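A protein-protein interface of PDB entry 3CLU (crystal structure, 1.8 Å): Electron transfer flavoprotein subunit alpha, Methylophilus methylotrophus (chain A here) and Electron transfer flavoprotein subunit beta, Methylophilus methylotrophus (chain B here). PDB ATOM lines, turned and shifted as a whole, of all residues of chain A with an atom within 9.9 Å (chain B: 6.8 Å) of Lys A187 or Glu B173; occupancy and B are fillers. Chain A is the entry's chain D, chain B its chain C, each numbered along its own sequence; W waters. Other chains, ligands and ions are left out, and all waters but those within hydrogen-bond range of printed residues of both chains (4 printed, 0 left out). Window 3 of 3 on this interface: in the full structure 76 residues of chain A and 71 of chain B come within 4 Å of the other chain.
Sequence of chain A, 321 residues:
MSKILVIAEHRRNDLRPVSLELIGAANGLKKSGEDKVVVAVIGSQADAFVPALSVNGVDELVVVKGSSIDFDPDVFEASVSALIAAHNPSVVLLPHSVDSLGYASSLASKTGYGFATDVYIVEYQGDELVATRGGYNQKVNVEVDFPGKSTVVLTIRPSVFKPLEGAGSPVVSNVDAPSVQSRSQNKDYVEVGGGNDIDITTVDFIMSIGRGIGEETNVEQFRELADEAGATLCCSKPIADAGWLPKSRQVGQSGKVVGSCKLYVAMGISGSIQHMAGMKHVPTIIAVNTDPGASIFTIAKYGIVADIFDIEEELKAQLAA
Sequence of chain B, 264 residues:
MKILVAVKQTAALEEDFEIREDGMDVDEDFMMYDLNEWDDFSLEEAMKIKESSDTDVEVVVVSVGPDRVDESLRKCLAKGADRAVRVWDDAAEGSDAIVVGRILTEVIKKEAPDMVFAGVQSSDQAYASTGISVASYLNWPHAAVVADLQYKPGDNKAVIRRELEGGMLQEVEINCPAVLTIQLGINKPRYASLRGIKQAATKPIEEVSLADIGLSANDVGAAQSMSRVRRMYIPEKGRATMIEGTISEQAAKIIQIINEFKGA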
ATOM      1  N   ARG A  12     -37.304  -9.777  -1.824  1.00  0.00           N
ATOM      2  CA  ARG A  12     -38.268  -9.008  -2.615  1.00  0.00           C
ATOM      3  C   ARG A  12     -39.657  -9.128  -2.028  1.00  0.00           C
ATOM      4  O   ARG A  12     -40.636  -9.335  -2.772  1.00  0.00           O
ATOM      5  CB  ARG A  12     -38.349  -9.519  -4.052  1.00  0.00           C
ATOM      6  CG  ARG A  12     -37.185  -9.210  -4.926  1.00  0.00           C
ATOM      7  CD  ARG A  12     -37.623  -9.250  -6.390  1.00  0.00           C
ATOM      8  NE  ARG A  12     -38.277 -10.506  -6.779  1.00  0.00           N
ATOM      9  CZ  ARG A  12     -38.627 -10.803  -8.031  1.00  0.00           C
ATOM     10  NH1 ARG A  12     -38.395  -9.948  -9.025  1.00  0.00           N
ATOM     11  NH2 ARG A  12     -39.209 -11.958  -8.299  1.00  0.00           N
ATOM     12  N   SER A  68     -30.113  -4.357   6.768  1.00  0.00           N
ATOM     13  CA  SER A  68     -30.506  -4.559   5.370  1.00  0.00           C
ATOM     14  C   SER A  68     -31.892  -5.125   5.255  1.00  0.00           C
ATOM     15  O   SER A  68     -32.393  -5.797   6.165  1.00  0.00           O
ATOM     16  CB  SER A  68     -29.514  -5.459   4.621  1.00  0.00           C
ATOM     17  OG  SER A  68     -29.365  -6.699   5.267  1.00  0.00           O
ATOM     18  N   ILE A  69     -32.512  -4.855   4.118  1.00  0.00           N
ATOM     19  CA  ILE A  69     -33.864  -5.343   3.817  1.00  0.00           C
ATOM     20  C   ILE A  69     -33.779  -6.831   3.581  1.00  0.00           C
ATOM     21  O   ILE A  69     -34.434  -7.603   4.291  1.00  0.00           O
ATOM     22  CB  ILE A  69     -34.487  -4.603   2.603  1.00  0.00           C
ATOM     23  CG1 ILE A  69     -34.735  -3.125   2.981  1.00  0.00           C
ATOM     24  CG2 ILE A  69     -35.784  -5.250   2.200  1.00  0.00           C
ATOM     25  CD1 ILE A  69     -35.084  -2.181   1.819  1.00  0.00           C
ATOM     26  N   ASP A  70     -32.914  -7.212   2.634  1.00  0.00           N
ATOM     27  CA  ASP A  70     -32.705  -8.600   2.251  1.00  0.00           C
ATOM     28  C   ASP A  70     -31.323  -9.096   2.678  1.00  0.00           C
ATOM     29  O   ASP A  70     -30.587  -8.398   3.382  1.00  0.00           O
ATOM     30  CB  ASP A  70     -32.946  -8.755   0.746  1.00  0.00           C
ATOM     31  CG  ASP A  70     -34.421  -8.740   0.384  1.00  0.00           C
ATOM     32  OD1 ASP A  70     -35.257  -8.885   1.303  1.00  0.00           O
ATOM     33  OD2 ASP A  70     -34.765  -8.619  -0.826  1.00  0.00           O
ATOM     34  N   PHE A  71     -30.981 -10.311   2.286  1.00  0.00           N
ATOM     35  CA  PHE A  71     -29.753 -10.910   2.715  1.00  0.00           C
ATOM     36  C   PHE A  71     -28.486 -10.060   2.592  1.00  0.00           C
ATOM     37  O   PHE A  71     -28.202  -9.447   1.561  1.00  0.00           O
ATOM     38  CB  PHE A  71     -29.514 -12.175   1.932  1.00  0.00           C
ATOM     39  CG  PHE A  71     -28.216 -12.801   2.265  1.00  0.00           C
ATOM     40  CD1 PHE A  71     -28.071 -13.474   3.476  1.00  0.00           C
ATOM     41  CD2 PHE A  71     -27.132 -12.695   1.404  1.00  0.00           C
ATOM     42  CE1 PHE A  71     -26.892 -14.057   3.821  1.00  0.00           C
ATOM     43  CE2 PHE A  71     -25.923 -13.284   1.747  1.00  0.00           C
ATOM     44  CZ  PHE A  71     -25.806 -13.949   2.965  1.00  0.00           C
ATOM     45  N   ASP A  72     -27.722 -10.060   3.662  1.00  0.00           N
ATOM     46  CA  ASP A  72     -26.422  -9.443   3.706  1.00  0.00           C
ATOM     47  C   ASP A  72     -25.580 -10.400   4.530  1.00  0.00           C
ATOM     48  O   ASP A  72     -25.972 -10.740   5.636  1.00  0.00           O
ATOM     49  CB  ASP A  72     -26.483  -8.106   4.416  1.00  0.00           C
ATOM     50  CG  ASP A  72     -25.096  -7.543   4.722  1.00  0.00           C
ATOM     51  OD1 ASP A  72     -24.386  -8.047   5.641  1.00  0.00           O
ATOM     52  OD2 ASP A  72     -24.703  -6.591   4.018  1.00  0.00           O
ATOM     53  N   PRO A  73     -24.423 -10.820   4.009  1.00  0.00           N
ATOM     54  CA  PRO A  73     -23.682 -11.862   4.738  1.00  0.00           C
ATOM     55  C   PRO A  73     -23.115 -11.450   6.114  1.00  0.00           C
ATOM     56  O   PRO A  73     -23.038 -12.298   6.995  1.00  0.00           O
ATOM     57  CB  PRO A  73     -22.547 -12.206   3.801  1.00  0.00           C
ATOM     58  CG  PRO A  73     -22.482 -11.164   2.787  1.00  0.00           C
ATOM     59  CD  PRO A  73     -23.710 -10.351   2.813  1.00  0.00           C
ATOM     60  N   ASP A  74     -22.706 -10.187   6.294  1.00  0.00           N
ATOM     61  CA  ASP A  74     -22.225  -9.743   7.603  1.00  0.00           C
ATOM     62  C   ASP A  74     -23.384  -9.670   8.608  1.00  0.00           C
ATOM     63  O   ASP A  74     -23.279 -10.170   9.727  1.00  0.00           O
ATOM     64  CB  ASP A  74     -21.489  -8.416   7.514  1.00  0.00           C
ATOM     65  CG  ASP A  74     -20.088  -8.569   6.954  1.00  0.00           C
ATOM     66  OD1 ASP A  74     -19.592  -9.722   6.794  1.00  0.00           O
ATOM     67  OD2 ASP A  74     -19.490  -7.524   6.666  1.00  0.00           O
ATOM     68  N   SER A 182     -21.951  -3.589   7.934  1.00  0.00           N
ATOM     69  CA  SER A 182     -21.622  -4.542   6.884  1.00  0.00           C
ATOM     70  C   SER A 182     -20.532  -4.004   5.969  1.00  0.00           C
ATOM     71  O   SER A 182     -20.456  -2.803   5.711  1.00  0.00           O
ATOM     72  CB  SER A 182     -22.834  -4.932   6.055  1.00  0.00           C
ATOM     73  OG  SER A 182     -22.451  -5.747   4.965  1.00  0.00           O
ATOM     74  N   ARG A 183     -19.715  -4.916   5.464  1.00  0.00           N
ATOM     75  CA  ARG A 183     -18.671  -4.560   4.529  1.00  0.00           C
ATOM     76  C   ARG A 183     -19.148  -4.595   3.059  1.00  0.00           C
ATOM     77  O   ARG A 183     -18.334  -4.443   2.126  1.00  0.00           O
ATOM     78  CB  ARG A 183     -17.443  -5.434   4.757  1.00  0.00           C
ATOM     79  CG  ARG A 183     -16.731  -5.092   6.067  1.00  0.00           C
ATOM     80  CD  ARG A 183     -15.817  -6.197   6.551  1.00  0.00           C
ATOM     81  NE  ARG A 183     -16.549  -7.428   6.718  1.00  0.00           N
ATOM     82  CZ  ARG A 183     -16.010  -8.569   7.123  1.00  0.00           C
ATOM     83  NH1 ARG A 183     -14.727  -8.633   7.400  1.00  0.00           N
ATOM     84  NH2 ARG A 183     -16.760  -9.638   7.243  1.00  0.00           N
ATOM     85  N   SER A 184     -20.463  -4.757   2.859  1.00  0.00           N
ATOM     86  CA  SER A 184     -21.067  -4.592   1.551  1.00  0.00           C
ATOM     87  C   SER A 184     -22.444  -3.948   1.676  1.00  0.00           C
ATOM     88  O   SER A 184     -23.022  -3.868   2.763  1.00  0.00           O
ATOM     89  CB  SER A 184     -21.146  -5.926   0.790  1.00  0.00           C
ATOM     90  OG  SER A 184     -21.940  -6.864   1.499  1.00  0.00           O
ATOM     91  N   GLN A 185     -22.906  -3.408   0.553  1.00  0.00           N
ATOM     92  CA  GLN A 185     -24.202  -2.805   0.444  1.00  0.00           C
ATOM     93  C   GLN A 185     -24.915  -3.365  -0.793  1.00  0.00           C
ATOM     94  O   GLN A 185     -24.375  -3.355  -1.893  1.00  0.00           O
ATOM     95  CB  GLN A 185     -24.020  -1.290   0.306  1.00  0.00           C
ATOM     96  CG  GLN A 185     -25.278  -0.528  -0.022  1.00  0.00           C
ATOM     97  CD  GLN A 185     -26.284  -0.461   1.116  1.00  0.00           C
ATOM     98  OE1 GLN A 185     -25.908  -0.391   2.300  1.00  0.00           O
ATOM     99  NE2 GLN A 185     -27.584  -0.454   0.759  1.00  0.00           N
ATOM    100  N   ASN A 186     -26.145  -3.804  -0.595  1.00  0.00           N
ATOM    101  CA  ASN A 186     -26.993  -4.315  -1.656  1.00  0.00           C
ATOM    102  C   ASN A 186     -27.501  -3.173  -2.509  1.00  0.00           C
ATOM    103  O   ASN A 186     -27.879  -2.126  -1.980  1.00  0.00           O
ATOM    104  CB  ASN A 186     -28.162  -5.058  -1.055  1.00  0.00           C
ATOM    105  CG  ASN A 186     -27.729  -6.311  -0.321  1.00  0.00           C
ATOM    106  OD1 ASN A 186     -26.633  -6.841  -0.567  1.00  0.00           O
ATOM    107  ND2 ASN A 186     -28.605  -6.823   0.544  1.00  0.00           N
ATOM    108  N   LYS A 187     -27.502  -3.383  -3.813  1.00  0.00           N
ATOM    109  CA  LYS A 187     -28.011  -2.417  -4.771  1.00  0.00           C
ATOM    110  C   LYS A 187     -29.170  -3.055  -5.550  1.00  0.00           C
ATOM    111  O   LYS A 187     -29.930  -3.832  -4.977  1.00  0.00           O
ATOM    112  CB  LYS A 187     -26.866  -1.902  -5.630  1.00  0.00           C
ATOM    113  CG  LYS A 187     -25.717  -1.326  -4.793  1.00  0.00           C
ATOM    114  CD  LYS A 187     -26.125  -0.061  -4.056  1.00  0.00           C
ATOM    115  CE  LYS A 187     -24.929   0.646  -3.386  1.00  0.00           C
ATOM    116  NZ  LYS A 187     -25.250   1.992  -2.810  1.00  0.00           N
ATOM    117  N   ASP A 188     -29.315  -2.762  -6.834  1.00  0.00           N
ATOM    118  CA  ASP A 188     -30.509  -3.208  -7.537  1.00  0.00           C
ATOM    119  C   ASP A 188     -30.563  -4.723  -7.660  1.00  0.00           C
ATOM    120  O   ASP A 188     -29.531  -5.381  -7.846  1.00  0.00           O
ATOM    121  CB  ASP A 188     -30.590  -2.614  -8.941  1.00  0.00           C
ATOM    122  CG  ASP A 188     -30.771  -1.120  -8.951  1.00  0.00           C
ATOM    123  OD1 ASP A 188     -31.420  -0.583  -8.041  1.00  0.00           O
ATOM    124  OD2 ASP A 188     -30.302  -0.483  -9.918  1.00  0.00           O
ATOM    125  N   TYR A 189     -31.773  -5.272  -7.598  1.00  0.00           N
ATOM    126  CA  TYR A 189     -32.010  -6.565  -8.255  1.00  0.00           C
ATOM    127  C   TYR A 189     -32.063  -6.347  -9.764  1.00  0.00           C
ATOM    128  O   TYR A 189     -32.486  -5.284 -10.242  1.00  0.00           O
ATOM    129  CB  TYR A 189     -33.300  -7.226  -7.777  1.00  0.00           C
ATOM    130  CG  TYR A 189     -33.233  -7.713  -6.360  1.00  0.00           C
ATOM    131  CD1 TYR A 189     -33.954  -7.093  -5.349  1.00  0.00           C
ATOM    132  CD2 TYR A 189     -32.428  -8.782  -6.021  1.00  0.00           C
ATOM    133  CE1 TYR A 189     -33.881  -7.544  -4.042  1.00  0.00           C
ATOM    134  CE2 TYR A 189     -32.344  -9.218  -4.751  1.00  0.00           C
ATOM    135  CZ  TYR A 189     -33.086  -8.611  -3.752  1.00  0.00           C
ATOM    136  OH  TYR A 189     -32.979  -9.052  -2.466  1.00  0.00           O
ATOM    137  N   VAL A 190     -31.672  -7.377 -10.519  1.00  0.00           N
ATOM    138  CA  VAL A 190     -31.536  -7.259 -11.959  1.00  0.00           C
ATOM    139  C   VAL A 190     -32.056  -8.511 -12.654  1.00  0.00           C
ATOM    140  O   VAL A 190     -31.835  -9.646 -12.186  1.00  0.00           O
ATOM    141  CB  VAL A 190     -30.046  -7.053 -12.364  1.00  0.00           C
ATOM    142  CG1 VAL A 190     -29.918  -6.892 -13.861  1.00  0.00           C
ATOM    143  CG2 VAL A 190     -29.441  -5.841 -11.635  1.00  0.00           C
ATOM    144  N   LYS B 157     -13.464  -0.459  -3.390  1.00  0.00           N
ATOM    145  CA  LYS B 157     -14.739  -1.153  -3.549  1.00  0.00           C
ATOM    146  C   LYS B 157     -14.897  -1.759  -4.958  1.00  0.00           C
ATOM    147  O   LYS B 157     -14.273  -1.319  -5.922  1.00  0.00           O
ATOM    148  CB  LYS B 157     -15.937  -0.259  -3.247  1.00  0.00           C
ATOM    149  CG  LYS B 157     -16.089   0.198  -1.773  1.00  0.00           C
ATOM    150  N   ALA B 158     -15.752  -2.768  -5.055  1.00  0.00           N
ATOM    151  CA  ALA B 158     -16.062  -3.419  -6.336  1.00  0.00           C
ATOM    152  C   ALA B 158     -17.566  -3.515  -6.394  1.00  0.00           C
ATOM    153  O   ALA B 158     -18.230  -3.404  -5.358  1.00  0.00           O
ATOM    154  CB  ALA B 158     -15.404  -4.829  -6.442  1.00  0.00           C
ATOM    155  N   VAL B 159     -18.109  -3.682  -7.591  1.00  0.00           N
ATOM    156  CA  VAL B 159     -19.511  -4.020  -7.729  1.00  0.00           C
ATOM    157  C   VAL B 159     -19.613  -5.390  -8.364  1.00  0.00           C
ATOM    158  O   VAL B 159     -19.050  -5.648  -9.446  1.00  0.00           O
ATOM    159  CB  VAL B 159     -20.300  -2.990  -8.553  1.00  0.00           C
ATOM    160  CG1 VAL B 159     -21.784  -3.452  -8.724  1.00  0.00           C
ATOM    161  CG2 VAL B 159     -20.224  -1.619  -7.893  1.00  0.00           C
ATOM    162  N   ILE B 160     -20.327  -6.276  -7.682  1.00  0.00           N
ATOM    163  CA  ILE B 160     -20.535  -7.621  -8.160  1.00  0.00           C
ATOM    164  C   ILE B 160     -21.988  -7.818  -8.400  1.00  0.00           C
ATOM    165  O   ILE B 160     -22.808  -7.075  -7.877  1.00  0.00           O
ATOM    166  CB  ILE B 160     -19.991  -8.711  -7.168  1.00  0.00           C
ATOM    167  CG1 ILE B 160     -20.622  -8.613  -5.766  1.00  0.00           C
ATOM    168  CG2 ILE B 160     -18.478  -8.576  -7.043  1.00  0.00           C
ATOM    169  CD1 ILE B 160     -21.765  -9.563  -5.506  1.00  0.00           C
ATOM    170  N   GLN B 170     -28.448  -9.903  -8.182  1.00  0.00           N
ATOM    171  CA  GLN B 170     -28.377  -8.779  -7.275  1.00  0.00           C
ATOM    172  C   GLN B 170     -27.026  -8.109  -7.353  1.00  0.00           C
ATOM    173  O   GLN B 170     -25.979  -8.753  -7.150  1.00  0.00           O
ATOM    174  CB  GLN B 170     -28.609  -9.202  -5.847  1.00  0.00           C
ATOM    175  CG  GLN B 170     -28.929  -8.035  -4.895  1.00  0.00           C
ATOM    176  CD  GLN B 170     -28.922  -8.500  -3.450  1.00  0.00           C
ATOM    177  OE1 GLN B 170     -28.190  -9.436  -3.085  1.00  0.00           O
ATOM    178  NE2 GLN B 170     -29.729  -7.886  -2.637  1.00  0.00           N
ATOM    179  N   GLU B 171     -27.069  -6.809  -7.623  1.00  0.00           N
ATOM    180  CA  GLU B 171     -25.880  -5.992  -7.553  1.00  0.00           C
ATOM    181  C   GLU B 171     -25.556  -5.727  -6.107  1.00  0.00           C
ATOM    182  O   GLU B 171     -26.439  -5.336  -5.304  1.00  0.00           O
ATOM    183  CB  GLU B 171     -26.071  -4.657  -8.252  1.00  0.00           C
ATOM    184  CG  GLU B 171     -26.388  -4.772  -9.684  1.00  0.00           C
ATOM    185  CD  GLU B 171     -26.020  -3.529 -10.439  1.00  0.00           C
ATOM    186  OE1 GLU B 171     -26.927  -2.755 -10.756  1.00  0.00           O
ATOM    187  OE2 GLU B 171     -24.809  -3.319 -10.680  1.00  0.00           O
ATOM    188  N   VAL B 172     -24.285  -5.881  -5.787  1.00  0.00           N
ATOM    189  CA  VAL B 172     -23.790  -5.641  -4.450  1.00  0.00           C
ATOM    190  C   VAL B 172     -22.505  -4.853  -4.559  1.00  0.00           C
ATOM    191  O   VAL B 172     -21.589  -5.274  -5.276  1.00  0.00           O
ATOM    192  CB  VAL B 172     -23.533  -6.981  -3.728  1.00  0.00           C
ATOM    193  CG1 VAL B 172     -22.874  -6.734  -2.371  1.00  0.00           C
ATOM    194  CG2 VAL B 172     -24.833  -7.720  -3.559  1.00  0.00           C
ATOM    195  N   GLU B 173     -22.426  -3.714  -3.873  1.00  0.00           N
ATOM    196  CA  GLU B 173     -21.137  -3.006  -3.748  1.00  0.00           C
ATOM    197  C   GLU B 173     -20.373  -3.585  -2.555  1.00  0.00           C
ATOM    198  O   GLU B 173     -20.902  -3.652  -1.459  1.00  0.00           O
ATOM    199  CB  GLU B 173     -21.363  -1.505  -3.595  1.00  0.00           C
ATOM    200  CG  GLU B 173     -20.073  -0.716  -3.479  1.00  0.00           C
ATOM    201  CD  GLU B 173     -20.320   0.755  -3.620  1.00  0.00           C
ATOM    202  OE1 GLU B 173     -19.799   1.350  -4.579  1.00  0.00           O
ATOM    203  OE2 GLU B 173     -21.069   1.282  -2.795  1.00  0.00           O
ATOM    204  N   ILE B 174     -19.133  -4.022  -2.769  1.00  0.00           N
ATOM    205  CA  ILE B 174     -18.379  -4.713  -1.729  1.00  0.00           C
ATOM    206  C   ILE B 174     -17.007  -4.078  -1.498  1.00  0.00           C
ATOM    207  O   ILE B 174     -16.308  -3.739  -2.442  1.00  0.00           O
ATOM    208  CB  ILE B 174     -18.256  -6.232  -2.060  1.00  0.00           C
ATOM    209  CG1 ILE B 174     -17.606  -7.000  -0.887  1.00  0.00           C
ATOM    210  CG2 ILE B 174     -17.549  -6.483  -3.403  1.00  0.00           C
ATOM    211  CD1 ILE B 174     -17.857  -8.486  -0.958  1.00  0.00           C
ATOM    212  N   ASN B 175     -16.653  -3.912  -0.225  1.00  0.00           N
ATOM    213  CA  ASN B 175     -15.345  -3.446   0.186  1.00  0.00           C
ATOM    214  C   ASN B 175     -14.260  -4.392  -0.288  1.00  0.00           C
ATOM    215  O   ASN B 175     -14.417  -5.613  -0.214  1.00  0.00           O
ATOM    216  CB  ASN B 175     -15.277  -3.353   1.705  1.00  0.00           C
ATOM    217  CG  ASN B 175     -16.077  -2.169   2.277  1.00  0.00           C
ATOM    218  OD1 ASN B 175     -16.142  -2.011   3.487  1.00  0.00           O
ATOM    219  ND2 ASN B 175     -16.661  -1.349   1.419  1.00  0.00           N
HETATM  220  O   HOH W   1     -28.787  -1.402 -11.884  1.00  0.00           O
HETATM  221  O   HOH W   2     -31.356  -5.793  -3.837  1.00  0.00           O
HETATM  222  O   HOH W   3     -27.857  -0.836  -8.550  1.00  0.00           O
HETATM  223  O   HOH W   4     -19.400  -1.604   0.868  1.00  0.00           O
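Among the printed residues, pairs that only touch across the chains: Arg A183 with Ile B174 (3.9 Å), Ser A184 with Val B172 (3.7 Å), Ser A184 with Glu B173 (3.2 Å), Ser A184 with Ile B174 (3.9 Å), Gln A185 with Val B172 (3.5 Å), Asn A186 with Gln B170 (3.4 Å), Asn A186 with Glu B171 (3.7 Å), Asn A186 with Val B172 (3.6 Å), Lys A187 with Glu B173 (3.96 Å), Asp A188 with Gln B170 (3.6 Å) and Val A190 with Glu B171 (3.8 Å).
Hydrophobic or aromatic side chains of chain B that line the printed part of chain A: Val B172.
Of the 17 printed residues of chain A, 8 touch a printed residue of chain B.
Hydrophobic or aromatic side chains of chain A that line the printed part of chain B: Tyr A189 and Val A190.
Among the printed residues, 16 pairs touch across the chains.
The backbone carbonyl oxygen (O) of Asp A188 lies within hydrogen-bond range of the backbone NH (N) of Glu B171, at 2.9 Å.
The side-chain hydroxyl of Tyr A189 sits at hydrogen-bond distance from the side-chain amide nitrogen of Gln B170 (3.5 Å).
The backbone NH (N) of Asn B175 sits at hydrogen-bond distance from the backbone carbonyl oxygen (O) of Arg A183, 2.9 Å away.
O of Glu B171 sits at hydrogen-bond distance from N of Lys A187 (2.7 Å).
N of Glu B173 is in hydrogen-bond range of O of Gln A185 (2.8 Å).
Water W1 bridges the side-chain carboxylate of Glu B171 (2.6 Å) and the side-chain carboxylate of Asp A188 (2.6 Å).
Water W2 lies within hydrogen-bond range of O of Lys A187 (2.7 Å) and NE2 of Gln B170 (2.9 Å).
Water W4 lies within hydrogen-bond range of ND2 of Asn B175 (2.8 Å), O of Arg A183 (3.3 Å) and O of Glu B173 (3.4 Å).
Water W3 bridges OD2 of Asp A188 (2.8 Å) and OE1 of Glu B171 (3.1 Å).
Ser A182 touches none of the printed residues of chain B.
Of the printed residues of chain B, Arg A183 touches Ile B174 (3.9 Å) and Asn B175 (2.9 Å).
Printed residues of chain B within 4 Å of Gln A185: Val B172 (3.5 Å) and Glu B173 (2.8 Å).
Printed residues of chain B within 4 Å of Asn A186: Gln B170, Glu B171 and Val B172.
Lys A187 touches just these residues of chain B: Glu B171 (2.7 Å) and Glu B173 (3.96 Å).
Of the printed residues of chain B, Asp A188 touches Gln B170 and Glu B171.
Ala B158 touches none of the printed residues of chain A.
Of the printed residues of chain A, Gln B170 touches Asn A186, Asp A188 and Tyr A189.
Glu B171 touches four residues of chain A.
Ile B174 touches just these residues of chain A: Arg A183 (3.9 Å) and Ser A184 (3.9 Å).
The nearest residue of chain B that does not touch Lys A187 is Gln B170 (4.3 Å).
OH of Tyr A189 sits at hydrogen-bond distance from OD2 of Asp A70, 2.5 Å away.
The backbone carbonyl oxygen (O) of Ala B158 sits at hydrogen-bond distance from the backbone NH (N) of Ile B174 (2.8 Å).
OG of Ser A182 sits at hydrogen-bond distance from O of Ser A184 (3.0 Å).
The guanidinium group (NH2) of Arg A183 is in salt-bridge range of the side-chain carboxylate (OD1) of Asp A74 (2.9 Å).
The backbone carbonyl oxygen of Ile B160 lies within hydrogen-bond range of the backbone NH of Val B172 (2.8 Å).
O of Phe A71 is in hydrogen-bond range of ND2 of Asn A186, at 2.8 Å.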
